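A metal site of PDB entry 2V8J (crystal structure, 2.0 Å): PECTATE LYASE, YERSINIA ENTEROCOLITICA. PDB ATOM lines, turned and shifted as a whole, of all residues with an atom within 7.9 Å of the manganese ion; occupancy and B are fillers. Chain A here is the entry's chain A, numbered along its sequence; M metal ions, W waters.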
ATOM      1  N   GLY A 104     -30.818  -9.178  16.374  1.00  0.00           N
ATOM      2  CA  GLY A 104     -30.266  -7.821  16.361  1.00  0.00           C
ATOM      3  C   GLY A 104     -31.177  -6.752  15.814  1.00  0.00           C
ATOM      4  O   GLY A 104     -31.093  -5.594  16.226  1.00  0.00           O
ATOM      5  N   HIS A 105     -32.064  -7.121  14.885  1.00  0.00           N
ATOM      6  CA  HIS A 105     -32.899  -6.118  14.225  1.00  0.00           C
ATOM      7  C   HIS A 105     -34.413  -6.401  14.172  1.00  0.00           C
ATOM      8  O   HIS A 105     -35.136  -5.687  13.469  1.00  0.00           O
ATOM      9  CB  HIS A 105     -32.392  -5.827  12.799  1.00  0.00           C
ATOM     10  CG  HIS A 105     -30.982  -5.363  12.752  1.00  0.00           C
ATOM     11  ND1 HIS A 105     -30.554  -4.187  13.346  1.00  0.00           N
ATOM     12  CD2 HIS A 105     -29.877  -5.907  12.180  1.00  0.00           C
ATOM     13  CE1 HIS A 105     -29.266  -4.035  13.129  1.00  0.00           C
ATOM     14  NE2 HIS A 105     -28.826  -5.075  12.440  1.00  0.00           N
ATOM     15  N   SER A 119     -34.886  -0.754  12.900  1.00  0.00           N
ATOM     16  CA  SER A 119     -33.935  -0.262  11.915  1.00  0.00           C
ATOM     17  C   SER A 119     -34.563  -0.430  10.532  1.00  0.00           C
ATOM     18  O   SER A 119     -34.596  -1.544  10.002  1.00  0.00           O
ATOM     19  CB  SER A 119     -32.607  -1.012  12.057  1.00  0.00           C
ATOM     20  OG  SER A 119     -31.598  -0.447  11.244  1.00  0.00           O
ATOM     21  N   GLU A 122     -32.861  -2.097   7.725  1.00  0.00           N
ATOM     22  CA  GLU A 122     -32.345  -3.406   8.154  1.00  0.00           C
ATOM     23  C   GLU A 122     -33.424  -4.270   8.820  1.00  0.00           C
ATOM     24  O   GLU A 122     -33.318  -4.600  10.010  1.00  0.00           O
ATOM     25  CB  GLU A 122     -31.166  -3.232   9.106  1.00  0.00           C
ATOM     26  CG  GLU A 122     -29.958  -2.450   8.542  1.00  0.00           C
ATOM     27  CD  GLU A 122     -28.994  -2.043   9.630  1.00  0.00           C
ATOM     28  OE1 GLU A 122     -29.466  -1.541  10.660  1.00  0.00           O
ATOM     29  OE2 GLU A 122     -27.765  -2.248   9.474  1.00  0.00           O
ATOM     30  N   VAL A 124     -34.146  -7.354   9.147  1.00  0.00           N
ATOM     31  CA  VAL A 124     -33.351  -8.555   8.882  1.00  0.00           C
ATOM     32  C   VAL A 124     -33.126  -9.391  10.139  1.00  0.00           C
ATOM     33  O   VAL A 124     -33.347  -8.937  11.259  1.00  0.00           O
ATOM     34  CB  VAL A 124     -31.952  -8.204   8.244  1.00  0.00           C
ATOM     35  CG1 VAL A 124     -32.098  -7.598   6.849  1.00  0.00           C
ATOM     36  CG2 VAL A 124     -31.124  -7.311   9.161  1.00  0.00           C
ATOM     37  N   HIS A 125     -32.667 -10.625   9.923  1.00  0.00           N
ATOM     38  CA  HIS A 125     -32.323 -11.541  11.008  1.00  0.00           C
ATOM     39  C   HIS A 125     -30.827 -11.451  11.290  1.00  0.00           C
ATOM     40  O   HIS A 125     -30.016 -11.541  10.373  1.00  0.00           O
ATOM     41  CB  HIS A 125     -32.697 -12.976  10.594  1.00  0.00           C
ATOM     42  CG  HIS A 125     -32.501 -13.994  11.669  1.00  0.00           C
ATOM     43  ND1 HIS A 125     -31.385 -14.799  11.728  1.00  0.00           N
ATOM     44  CD2 HIS A 125     -33.286 -14.375  12.711  1.00  0.00           C
ATOM     45  CE1 HIS A 125     -31.485 -15.623  12.758  1.00  0.00           C
ATOM     46  NE2 HIS A 125     -32.632 -15.396  13.368  1.00  0.00           N
ATOM     47  N   GLU A 126     -30.486 -11.263  12.553  1.00  0.00           N
ATOM     48  CA  GLU A 126     -29.099 -11.243  12.984  1.00  0.00           C
ATOM     49  C   GLU A 126     -28.950 -11.870  14.371  1.00  0.00           C
ATOM     50  O   GLU A 126     -29.740 -11.583  15.275  1.00  0.00           O
ATOM     51  CB  GLU A 126     -28.529  -9.801  12.958  1.00  0.00           C
ATOM     52  CG  GLU A 126     -27.097  -9.659  13.556  1.00  0.00           C
ATOM     53  CD  GLU A 126     -26.420  -8.337  13.195  1.00  0.00           C
ATOM     54  OE1 GLU A 126     -27.138  -7.384  12.903  1.00  0.00           O
ATOM     55  OE2 GLU A 126     -25.161  -8.250  13.199  1.00  0.00           O
ATOM     56  N   LEU A 127     -27.948 -12.749  14.500  1.00  0.00           N
ATOM     57  CA  LEU A 127     -27.536 -13.333  15.783  1.00  0.00           C
ATOM     58  C   LEU A 127     -26.029 -13.228  15.967  1.00  0.00           C
ATOM     59  O   LEU A 127     -25.261 -13.766  15.165  1.00  0.00           O
ATOM     60  CB  LEU A 127     -28.005 -14.803  15.961  1.00  0.00           C
ATOM     61  CG  LEU A 127     -29.510 -15.126  15.914  1.00  0.00           C
ATOM     62  CD1 LEU A 127     -29.757 -16.629  15.891  1.00  0.00           C
ATOM     63  CD2 LEU A 127     -30.295 -14.470  17.045  1.00  0.00           C
ATOM     64  N   ARG A 167     -23.689 -11.313   8.136  1.00  0.00           N
ATOM     65  CA  ARG A 167     -24.280 -10.906   9.427  1.00  0.00           C
ATOM     66  C   ARG A 167     -25.812 -10.767   9.391  1.00  0.00           C
ATOM     67  O   ARG A 167     -26.499 -11.104  10.360  1.00  0.00           O
ATOM     68  CB  ARG A 167     -23.658  -9.598   9.933  1.00  0.00           C
ATOM     69  CG  ARG A 167     -22.484  -9.823  10.888  1.00  0.00           C
ATOM     70  CD  ARG A 167     -21.678  -8.553  11.156  1.00  0.00           C
ATOM     71  NE  ARG A 167     -20.575  -8.789  12.098  1.00  0.00           N
ATOM     72  CZ  ARG A 167     -19.564  -7.955  12.309  1.00  0.00           C
ATOM     73  NH1 ARG A 167     -19.465  -6.795  11.653  1.00  0.00           N
ATOM     74  NH2 ARG A 167     -18.612  -8.283  13.190  1.00  0.00           N
ATOM     75  N   HIS A 168     -26.334 -10.287   8.269  1.00  0.00           N
ATOM     76  CA  HIS A 168     -27.753 -10.054   8.086  1.00  0.00           C
ATOM     77  C   HIS A 168     -28.349 -11.169   7.238  1.00  0.00           C
ATOM     78  O   HIS A 168     -27.767 -11.564   6.240  1.00  0.00           O
ATOM     79  CB  HIS A 168     -27.970  -8.710   7.387  1.00  0.00           C
ATOM     80  CG  HIS A 168     -27.724  -7.525   8.274  1.00  0.00           C
ATOM     81  ND1 HIS A 168     -27.929  -6.227   7.862  1.00  0.00           N
ATOM     82  CD2 HIS A 168     -27.308  -7.457   9.564  1.00  0.00           C
ATOM     83  CE1 HIS A 168     -27.627  -5.411   8.850  1.00  0.00           C
ATOM     84  NE2 HIS A 168     -27.256  -6.128   9.895  1.00  0.00           N
ATOM     85  N   PHE A 509     -29.144  -8.632  21.797  1.00  0.00           N
ATOM     86  CA  PHE A 509     -29.108  -7.163  21.645  1.00  0.00           C
ATOM     87  C   PHE A 509     -30.157  -6.749  20.616  1.00  0.00           C
ATOM     88  O   PHE A 509     -30.594  -7.558  19.807  1.00  0.00           O
ATOM     89  CB  PHE A 509     -27.702  -6.673  21.240  1.00  0.00           C
ATOM     90  CG  PHE A 509     -27.376  -6.820  19.756  1.00  0.00           C
ATOM     91  CD1 PHE A 509     -27.353  -5.709  18.918  1.00  0.00           C
ATOM     92  CD2 PHE A 509     -27.089  -8.072  19.214  1.00  0.00           C
ATOM     93  CE1 PHE A 509     -27.041  -5.827  17.555  1.00  0.00           C
ATOM     94  CE2 PHE A 509     -26.774  -8.211  17.843  1.00  0.00           C
ATOM     95  CZ  PHE A 509     -26.750  -7.089  17.013  1.00  0.00           C
ATOM     96  N   GLU A 511     -30.913  -3.392  17.928  1.00  0.00           N
ATOM     97  CA  GLU A 511     -30.259  -2.228  17.338  1.00  0.00           C
ATOM     98  C   GLU A 511     -31.108  -1.534  16.282  1.00  0.00           C
ATOM     99  O   GLU A 511     -31.633  -2.177  15.368  1.00  0.00           O
ATOM    100  CB  GLU A 511     -28.903  -2.601  16.740  1.00  0.00           C
ATOM    101  CG  GLU A 511     -28.053  -1.421  16.277  1.00  0.00           C
ATOM    102  CD  GLU A 511     -26.764  -1.870  15.634  1.00  0.00           C
ATOM    103  OE1 GLU A 511     -26.774  -2.223  14.445  1.00  0.00           O
ATOM    104  OE2 GLU A 511     -25.724  -1.875  16.314  1.00  0.00           O
HETATM  105 MN    MN M   1     -26.836  -5.474  11.941  1.00  0.00          MN
HETATM  106  O   HOH W   1     -26.264  -3.509  11.403  1.00  0.00           O
HETATM  107  O   HOH W   2     -24.766  -5.765  11.664  1.00  0.00           O
HETATM  108  O   HOH W   3     -25.992  -4.826  13.665  1.00  0.00           O
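A ring nitrogen (ND1) of His 105 is in hydrogen-bond range of the backbone carbonyl oxygen of Glu 511 (3.0 Å). N of Gly 104 lies within hydrogen-bond range of O of Glu 126 (2.9 Å).
Three residues have an atom within 4 Å of the manganese ion: His 105, Glu 126 and His 168. The nearest printed residue that does not touch the manganese ion is Glu 511 (4.1 Å).
The manganese ion is bound by water W3, NE2 of His 105, water W2, water W1, OE1 of Glu 126 and NE2 of His 168. The manganese ion has six donor atoms within binding distance.
Water W1 bridges the side-chain carboxylate of Glu 122 (2.8 Å) and the side-chain carboxylate of Glu 511 (3.3 Å).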
